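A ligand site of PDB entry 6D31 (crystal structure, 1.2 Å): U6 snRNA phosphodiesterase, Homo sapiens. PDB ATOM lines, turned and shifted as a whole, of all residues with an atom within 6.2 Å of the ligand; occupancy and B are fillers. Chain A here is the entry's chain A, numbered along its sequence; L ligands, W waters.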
ATOM      1  N   HIS A  10     -26.679 -30.856   6.749  1.00  0.00           N
ATOM      2  CA  HIS A  10     -27.260 -30.398   8.019  1.00  0.00           C
ATOM      3  C   HIS A  10     -28.707 -30.865   8.023  1.00  0.00           C
ATOM      4  O   HIS A  10     -29.386 -30.756   7.046  1.00  0.00           O
ATOM      5  CB  HIS A  10     -27.207 -28.892   8.032  1.00  0.00           C
ATOM      6  CG  HIS A  10     -27.698 -28.242   9.272  1.00  0.00           C
ATOM      7  ND1 HIS A  10     -28.236 -26.989   9.213  1.00  0.00           N
ATOM      8  CD2 HIS A  10     -27.717 -28.588  10.553  1.00  0.00           C
ATOM      9  CE1 HIS A  10     -28.553 -26.571  10.407  1.00  0.00           C
ATOM     10  NE2 HIS A  10     -28.285 -27.536  11.249  1.00  0.00           N
ATOM     11  N   MET A  42     -32.672 -14.121  10.429  1.00  0.00           N
ATOM     12  CA  MET A  42     -32.535 -15.330   9.645  1.00  0.00           C
ATOM     13  C   MET A  42     -33.487 -15.272   8.452  1.00  0.00           C
ATOM     14  O   MET A  42     -34.546 -14.664   8.521  1.00  0.00           O
ATOM     15  CB  MET A  42     -32.996 -16.509  10.457  1.00  0.00           C
ATOM     16  CG  MET A  42     -31.938 -17.299  11.030  1.00  0.00           C
ATOM     17  SD  MET A  42     -30.729 -16.531  12.106  1.00  0.00           S
ATOM     18  CE  MET A  42     -29.475 -17.679  11.876  1.00  0.00           C
ATOM     19  N   HIS A  46     -35.233 -22.812  11.429  1.00  0.00           N
ATOM     20  CA  HIS A  46     -34.970 -24.236  11.587  1.00  0.00           C
ATOM     21  C   HIS A  46     -34.687 -24.523  13.048  1.00  0.00           C
ATOM     22  O   HIS A  46     -34.235 -23.640  13.787  1.00  0.00           O
ATOM     23  CB  HIS A  46     -33.759 -24.665  10.717  1.00  0.00           C
ATOM     24  CG  HIS A  46     -32.466 -24.028  11.150  1.00  0.00           C
ATOM     25  ND1 HIS A  46     -32.051 -22.794  10.690  1.00  0.00           N
ATOM     26  CD2 HIS A  46     -31.496 -24.441  12.018  1.00  0.00           C
ATOM     27  CE1 HIS A  46     -30.910 -22.461  11.269  1.00  0.00           C
ATOM     28  NE2 HIS A  46     -30.555 -23.432  12.085  1.00  0.00           N
ATOM     29  N   LEU A  47     -34.901 -25.798  13.456  1.00  0.00           N
ATOM     30  CA  LEU A  47     -34.357 -26.313  14.696  1.00  0.00           C
ATOM     31  C   LEU A  47     -33.426 -27.452  14.322  1.00  0.00           C
ATOM     32  O   LEU A  47     -33.870 -28.485  13.798  1.00  0.00           O
ATOM     33  CB  LEU A  47     -35.412 -26.770  15.698  1.00  0.00           C
ATOM     34  CG  LEU A  47     -36.333 -25.627  16.036  1.00  0.00           C
ATOM     35  CD1 LEU A  47     -37.593 -25.686  15.271  1.00  0.00           C
ATOM     36  CD2 LEU A  47     -36.683 -25.680  17.519  1.00  0.00           C
ATOM     37  N   SER A  48     -32.151 -27.265  14.541  1.00  0.00           N
ATOM     38  CA  SER A  48     -31.142 -28.248  14.182  1.00  0.00           C
ATOM     39  C   SER A  48     -31.311 -29.592  14.906  1.00  0.00           C
ATOM     40  O   SER A  48     -31.506 -29.621  16.106  1.00  0.00           O
ATOM     41  CB  SER A  48     -29.755 -27.698  14.413  1.00  0.00           C
ATOM     42  OG  SER A  48     -29.573 -26.630  13.517  1.00  0.00           O
ATOM     43  N   SER A  50     -28.690 -31.869  13.775  1.00  0.00           N
ATOM     44  CA  SER A  50     -27.340 -32.323  13.574  1.00  0.00           C
ATOM     45  C   SER A  50     -26.441 -31.098  13.556  1.00  0.00           C
ATOM     46  O   SER A  50     -26.925 -29.954  13.444  1.00  0.00           O
ATOM     47  CB  SER A  50     -27.185 -33.062  12.235  1.00  0.00           C
ATOM     48  OG  SER A  50     -27.111 -32.178  11.133  1.00  0.00           O
ATOM     49  N   TYR A  87     -26.878 -17.732  21.836  1.00  0.00           N
ATOM     50  CA  TYR A  87     -25.981 -18.791  21.465  1.00  0.00           C
ATOM     51  C   TYR A  87     -24.794 -18.207  20.758  1.00  0.00           C
ATOM     52  O   TYR A  87     -24.925 -17.189  20.080  1.00  0.00           O
ATOM     53  CB  TYR A  87     -26.627 -19.813  20.497  1.00  0.00           C
ATOM     54  CG  TYR A  87     -27.796 -20.490  21.134  1.00  0.00           C
ATOM     55  CD1 TYR A  87     -27.620 -21.725  21.766  1.00  0.00           C
ATOM     56  CD2 TYR A  87     -29.087 -19.971  21.079  1.00  0.00           C
ATOM     57  CE1 TYR A  87     -28.707 -22.392  22.330  1.00  0.00           C
ATOM     58  CE2 TYR A  87     -30.183 -20.675  21.629  1.00  0.00           C
ATOM     59  CZ  TYR A  87     -29.926 -21.872  22.301  1.00  0.00           C
ATOM     60  OH  TYR A  87     -31.040 -22.544  22.779  1.00  0.00           O
ATOM     61  N   THR A  88     -23.660 -18.868  20.870  1.00  0.00           N
ATOM     62  CA  THR A  88     -22.536 -18.620  19.989  1.00  0.00           C
ATOM     63  C   THR A  88     -22.192 -19.938  19.305  1.00  0.00           C
ATOM     64  O   THR A  88     -22.470 -21.039  19.794  1.00  0.00           O
ATOM     65  CB  THR A  88     -21.289 -18.090  20.683  1.00  0.00           C
ATOM     66  OG1 THR A  88     -20.953 -18.984  21.746  1.00  0.00           O
ATOM     67  CG2 THR A  88     -21.541 -16.762  21.308  1.00  0.00           C
ATOM     68  N   ASN A  89     -21.590 -19.809  18.139  1.00  0.00           N
ATOM     69  CA  ASN A  89     -20.959 -20.976  17.576  1.00  0.00           C
ATOM     70  C   ASN A  89     -19.718 -21.352  18.405  1.00  0.00           C
ATOM     71  O   ASN A  89     -19.337 -20.667  19.374  1.00  0.00           O
ATOM     72  CB  ASN A  89     -20.636 -20.796  16.091  1.00  0.00           C
ATOM     73  CG  ASN A  89     -19.612 -19.694  15.841  1.00  0.00           C
ATOM     74  OD1 ASN A  89     -19.103 -19.055  16.781  1.00  0.00           O
ATOM     75  ND2 ASN A  89     -19.292 -19.522  14.600  1.00  0.00           N
ATOM     76  N   GLN A  90     -19.115 -22.475  18.025  1.00  0.00           N
ATOM     77  CA  GLN A  90     -18.039 -22.996  18.875  1.00  0.00           C
ATOM     78  C   GLN A  90     -16.838 -22.057  18.932  1.00  0.00           C
ATOM     79  O   GLN A  90     -16.210 -21.927  19.988  1.00  0.00           O
ATOM     80  CB  GLN A  90     -17.663 -24.401  18.397  1.00  0.00           C
ATOM     81  CG  GLN A  90     -16.414 -24.995  18.958  1.00  0.00           C
ATOM     82  CD  GLN A  90     -16.133 -26.385  18.342  1.00  0.00           C
ATOM     83  OE1 GLN A  90     -17.076 -27.121  17.984  1.00  0.00           O
ATOM     84  NE2 GLN A  90     -14.867 -26.740  18.229  1.00  0.00           N
ATOM     85  N   PHE A  96     -26.038 -15.721  18.088  1.00  0.00           N
ATOM     86  CA  PHE A  96     -27.382 -15.945  17.661  1.00  0.00           C
ATOM     87  C   PHE A  96     -28.331 -15.607  18.798  1.00  0.00           C
ATOM     88  O   PHE A  96     -28.049 -15.904  19.954  1.00  0.00           O
ATOM     89  CB  PHE A  96     -27.640 -17.435  17.284  1.00  0.00           C
ATOM     90  CG  PHE A  96     -26.725 -17.945  16.236  1.00  0.00           C
ATOM     91  CD1 PHE A  96     -27.092 -17.982  14.900  1.00  0.00           C
ATOM     92  CD2 PHE A  96     -25.449 -18.331  16.564  1.00  0.00           C
ATOM     93  CE1 PHE A  96     -26.208 -18.429  13.938  1.00  0.00           C
ATOM     94  CE2 PHE A  96     -24.583 -18.749  15.580  1.00  0.00           C
ATOM     95  CZ  PHE A  96     -24.985 -18.814  14.290  1.00  0.00           C
ATOM     96  N   PHE A 127     -24.576 -35.187  17.301  1.00  0.00           N
ATOM     97  CA  PHE A 127     -25.001 -33.863  17.772  1.00  0.00           C
ATOM     98  C   PHE A 127     -24.360 -33.591  19.138  1.00  0.00           C
ATOM     99  O   PHE A 127     -23.856 -34.495  19.846  1.00  0.00           O
ATOM    100  CB  PHE A 127     -26.535 -33.799  17.880  1.00  0.00           C
ATOM    101  CG  PHE A 127     -27.120 -32.392  17.847  1.00  0.00           C
ATOM    102  CD1 PHE A 127     -26.731 -31.454  16.895  1.00  0.00           C
ATOM    103  CD2 PHE A 127     -28.071 -32.034  18.779  1.00  0.00           C
ATOM    104  CE1 PHE A 127     -27.333 -30.198  16.869  1.00  0.00           C
ATOM    105  CE2 PHE A 127     -28.664 -30.769  18.689  1.00  0.00           C
ATOM    106  CZ  PHE A 127     -28.256 -29.859  17.723  1.00  0.00           C
ATOM    107  N   TYR A 128     -24.465 -32.357  19.564  1.00  0.00           N
ATOM    108  CA  TYR A 128     -23.954 -31.997  20.895  1.00  0.00           C
ATOM    109  C   TYR A 128     -24.516 -32.886  21.971  1.00  0.00           C
ATOM    110  O   TYR A 128     -25.678 -33.220  21.927  1.00  0.00           O
ATOM    111  CB  TYR A 128     -24.418 -30.559  21.167  1.00  0.00           C
ATOM    112  CG  TYR A 128     -24.021 -29.638  20.060  1.00  0.00           C
ATOM    113  CD1 TYR A 128     -22.666 -29.433  19.746  1.00  0.00           C
ATOM    114  CD2 TYR A 128     -24.950 -29.083  19.219  1.00  0.00           C
ATOM    115  CE1 TYR A 128     -22.296 -28.638  18.701  1.00  0.00           C
ATOM    116  CE2 TYR A 128     -24.591 -28.286  18.182  1.00  0.00           C
ATOM    117  CZ  TYR A 128     -23.256 -28.055  17.932  1.00  0.00           C
ATOM    118  OH  TYR A 128     -22.933 -27.243  16.914  1.00  0.00           O
ATOM    119  N   ASP A 130     -24.942 -32.031  25.098  1.00  0.00           N
ATOM    120  CA  ASP A 130     -25.770 -31.167  25.918  1.00  0.00           C
ATOM    121  C   ASP A 130     -26.591 -30.302  24.977  1.00  0.00           C
ATOM    122  O   ASP A 130     -26.453 -29.077  24.944  1.00  0.00           O
ATOM    123  CB  ASP A 130     -24.915 -30.283  26.836  1.00  0.00           C
ATOM    124  CG  ASP A 130     -23.931 -31.059  27.696  1.00  0.00           C
ATOM    125  OD1 ASP A 130     -24.202 -32.235  27.945  1.00  0.00           O
ATOM    126  OD2 ASP A 130     -22.906 -30.467  28.137  1.00  0.00           O
ATOM    127  N   PRO A 131     -27.463 -30.890  24.169  1.00  0.00           N
ATOM    128  CA  PRO A 131     -28.154 -30.107  23.163  1.00  0.00           C
ATOM    129  C   PRO A 131     -29.124 -29.134  23.765  1.00  0.00           C
ATOM    130  O   PRO A 131     -29.811 -29.421  24.736  1.00  0.00           O
ATOM    131  CB  PRO A 131     -28.851 -31.141  22.324  1.00  0.00           C
ATOM    132  CG  PRO A 131     -29.137 -32.177  23.274  1.00  0.00           C
ATOM    133  CD  PRO A 131     -27.902 -32.291  24.142  1.00  0.00           C
ATOM    134  N   SER A 132     -29.196 -27.966  23.137  1.00  0.00           N
ATOM    135  CA  SER A 132     -30.174 -26.951  23.495  1.00  0.00           C
ATOM    136  C   SER A 132     -30.909 -26.666  22.216  1.00  0.00           C
ATOM    137  O   SER A 132     -30.408 -25.938  21.384  1.00  0.00           O
ATOM    138  CB  SER A 132     -29.489 -25.751  24.071  1.00  0.00           C
ATOM    139  OG  SER A 132     -30.408 -24.706  24.231  1.00  0.00           O
ATOM    140  N   PHE A 133     -32.053 -27.225  22.017  1.00  0.00           N
ATOM    141  CA  PHE A 133     -32.750 -27.106  20.754  1.00  0.00           C
ATOM    142  C   PHE A 133     -33.333 -25.705  20.713  1.00  0.00           C
ATOM    143  O   PHE A 133     -33.814 -25.175  21.719  1.00  0.00           O
ATOM    144  CB  PHE A 133     -33.882 -28.139  20.712  1.00  0.00           C
ATOM    145  CG  PHE A 133     -33.356 -29.522  20.694  1.00  0.00           C
ATOM    146  CD1 PHE A 133     -32.766 -30.054  19.568  1.00  0.00           C
ATOM    147  CD2 PHE A 133     -33.315 -30.273  21.869  1.00  0.00           C
ATOM    148  CE1 PHE A 133     -32.216 -31.308  19.546  1.00  0.00           C
ATOM    149  CE2 PHE A 133     -32.766 -31.554  21.828  1.00  0.00           C
ATOM    150  CZ  PHE A 133     -32.229 -32.052  20.718  1.00  0.00           C
ATOM    151  N   HIS A 134     -33.294 -25.115  19.524  1.00  0.00           N
ATOM    152  CA  HIS A 134     -33.725 -23.733  19.466  1.00  0.00           C
ATOM    153  C   HIS A 134     -34.001 -23.368  18.041  1.00  0.00           C
ATOM    154  O   HIS A 134     -33.471 -23.956  17.093  1.00  0.00           O
ATOM    155  CB  HIS A 134     -32.647 -22.763  19.981  1.00  0.00           C
ATOM    156  CG  HIS A 134     -31.347 -22.874  19.302  1.00  0.00           C
ATOM    157  ND1 HIS A 134     -30.431 -23.871  19.578  1.00  0.00           N
ATOM    158  CD2 HIS A 134     -30.828 -22.192  18.251  1.00  0.00           C
ATOM    159  CE1 HIS A 134     -29.370 -23.731  18.801  1.00  0.00           C
ATOM    160  NE2 HIS A 134     -29.605 -22.741  17.963  1.00  0.00           N
ATOM    161  N   LEU A 135     -34.776 -22.296  17.926  1.00  0.00           N
ATOM    162  CA  LEU A 135     -35.040 -21.632  16.663  1.00  0.00           C
ATOM    163  C   LEU A 135     -34.247 -20.337  16.699  1.00  0.00           C
ATOM    164  O   LEU A 135     -34.610 -19.412  17.434  1.00  0.00           O
ATOM    165  CB  LEU A 135     -36.541 -21.256  16.738  1.00  0.00           C
ATOM    166  CG  LEU A 135     -37.176 -20.616  15.593  1.00  0.00           C
ATOM    167  CD1 LEU A 135     -37.004 -21.497  14.419  1.00  0.00           C
ATOM    168  CD2 LEU A 135     -38.591 -20.290  15.741  1.00  0.00           C
ATOM    169  N   SER A 136     -33.190 -20.254  15.931  1.00  0.00           N
ATOM    170  CA  SER A 136     -32.458 -18.988  15.805  1.00  0.00           C
ATOM    171  C   SER A 136     -33.273 -17.980  15.051  1.00  0.00           C
ATOM    172  O   SER A 136     -33.884 -18.273  14.041  1.00  0.00           O
ATOM    173  CB  SER A 136     -31.132 -19.184  15.101  1.00  0.00           C
ATOM    174  OG  SER A 136     -30.293 -19.931  15.972  1.00  0.00           O
HETATM  175  P1  LIG L   1     -28.363 -23.168  14.653  1.00  0.00           P
HETATM  176  O1  LIG L   1     -28.927 -24.523  14.978  1.00  0.00           O
HETATM  177  O2  LIG L   1     -27.472 -23.164  13.457  1.00  0.00           O
HETATM  178  O3  LIG L   1     -29.335 -22.067  14.551  1.00  0.00           O
HETATM  179  O4  LIG L   1     -27.477 -22.837  15.949  1.00  0.00           O
HETATM  180  C1  LIG L   1     -26.647 -21.703  16.045  1.00  0.00           C
HETATM  181  C2  LIG L   1     -25.436 -22.113  16.818  1.00  0.00           C
HETATM  182  O5  LIG L   1     -25.811 -22.528  18.127  1.00  0.00           O
HETATM  183  C3  LIG L   1     -24.611 -23.269  16.264  1.00  0.00           C
HETATM  184  O6  LIG L   1     -23.393 -22.765  15.734  1.00  0.00           O
HETATM  185  C4  LIG L   1     -24.321 -24.123  17.496  1.00  0.00           C
HETATM  186  O7  LIG L   1     -22.979 -24.473  17.648  1.00  0.00           O
HETATM  187  C5  LIG L   1     -24.737 -23.227  18.609  1.00  0.00           C
HETATM  188  N1  LIG L   1     -25.016 -23.853  19.880  1.00  0.00           N
HETATM  189  C6  LIG L   1     -24.374 -23.499  21.002  1.00  0.00           C
HETATM  190  N2  LIG L   1     -24.673 -24.287  22.009  1.00  0.00           N
HETATM  191  C7  LIG L   1     -25.567 -25.176  21.518  1.00  0.00           C
HETATM  192  C8  LIG L   1     -26.214 -26.300  22.052  1.00  0.00           C
HETATM  193  N3  LIG L   1     -25.975 -26.602  23.346  1.00  0.00           N
HETATM  194  N4  LIG L   1     -27.075 -26.998  21.280  1.00  0.00           N
HETATM  195  C9  LIG L   1     -27.234 -26.654  20.013  1.00  0.00           C
HETATM  196  N5  LIG L   1     -26.595 -25.666  19.358  1.00  0.00           N
HETATM  197  C10 LIG L   1     -25.807 -24.970  20.175  1.00  0.00           C
HETATM  198  O   HOH W   1     -23.580 -26.194  24.716  1.00  0.00           O
HETATM  199  O   HOH W   2     -27.471 -26.242  16.647  1.00  0.00           O
HETATM  200  O   HOH W   3     -31.953 -22.234  14.387  1.00  0.00           O
HETATM  201  O   HOH W   4     -26.633 -26.948  26.687  1.00  0.00           O
HETATM  202  O   HOH W   5     -27.968 -20.907  11.651  1.00  0.00           O
HETATM  203  O   HOH W   6     -20.593 -24.240  16.080  1.00  0.00           O
HETATM  204  O   HOH W   7     -31.216 -25.044  16.051  1.00  0.00           O
HETATM  205  O   HOH W   8     -21.170 -24.210  20.136  1.00  0.00           O
HETATM  206  O   HOH W   9     -26.012 -25.351  12.664  1.00  0.00           O
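An oxygen (O3) of the ligand is in hydrogen-bond range of a ring nitrogen (NE2) of His 46 (3.1 Å).
O3 of the ligand lies within hydrogen-bond range of OG of Ser 136, at 2.7 Å.
The side-chain hydroxyl (OG) of Ser 48 lies within hydrogen-bond range of an oxygen (O1) of the ligand (2.6 Å).
N of Ser 132 is in hydrogen-bond range of N4 of the ligand.
The side-chain hydroxyl of Tyr 128 is in hydrogen-bond range of an oxygen (O7) of the ligand (2.9 Å).
An oxygen (O4) of the ligand is in hydrogen-bond range of a ring nitrogen (NE2) of His 134 (2.9 Å).
A nitrogen (N3) of the ligand is in hydrogen-bond range of the backbone carbonyl oxygen of Asp 130, 3.0 Å away.
The backbone NH (N) of Phe 96 is in hydrogen-bond range of the backbone carbonyl oxygen (O) of Tyr 87, 2.7 Å away.
A ring nitrogen (ND1) of His 134 is in hydrogen-bond range of the backbone carbonyl oxygen (O) of Ser 132 (2.7 Å).
OG of Ser 132 lies within hydrogen-bond range of OH of Tyr 87, at 2.7 Å.
OG of Ser 48 sits at hydrogen-bond distance from NE2 of His 10, 2.8 Å away.
Merely in contact with the ligand: Tyr 87, Thr 88, Asn 89, Phe 96 and Pro 131.
Hydrophobic or aromatic side chains within 4 Å of the ligand: His 46, Tyr 87, Phe 96, Tyr 128 and His 134.
Water W7 lies within hydrogen-bond range of O1 of the ligand (2.6 Å), O of His 134 (2.7 Å) and N of Ser 48 (2.8 Å).
Water W3 lies within hydrogen-bond range of an oxygen (O3) of the ligand (2.6 Å), the backbone carbonyl oxygen (O) of His 46 (2.7 Å) and the backbone NH (N) of Ser 136 (2.8 Å).
Water W9 lies within hydrogen-bond range of O2 of the ligand (2.7 Å) and NE2 of His 10 (3.5 Å).
Water W6 bridges an oxygen (O7) of the ligand and the backbone NH of Gln 90.
Water W8 lies within hydrogen-bond range of O7 of the ligand (3.1 Å), N of Gln 90 (3.4 Å) and O of Thr 88 (3.4 Å).
Water W4 lies within hydrogen-bond range of O of Asp 130 (2.8 Å) and N3 of the ligand (3.4 Å).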
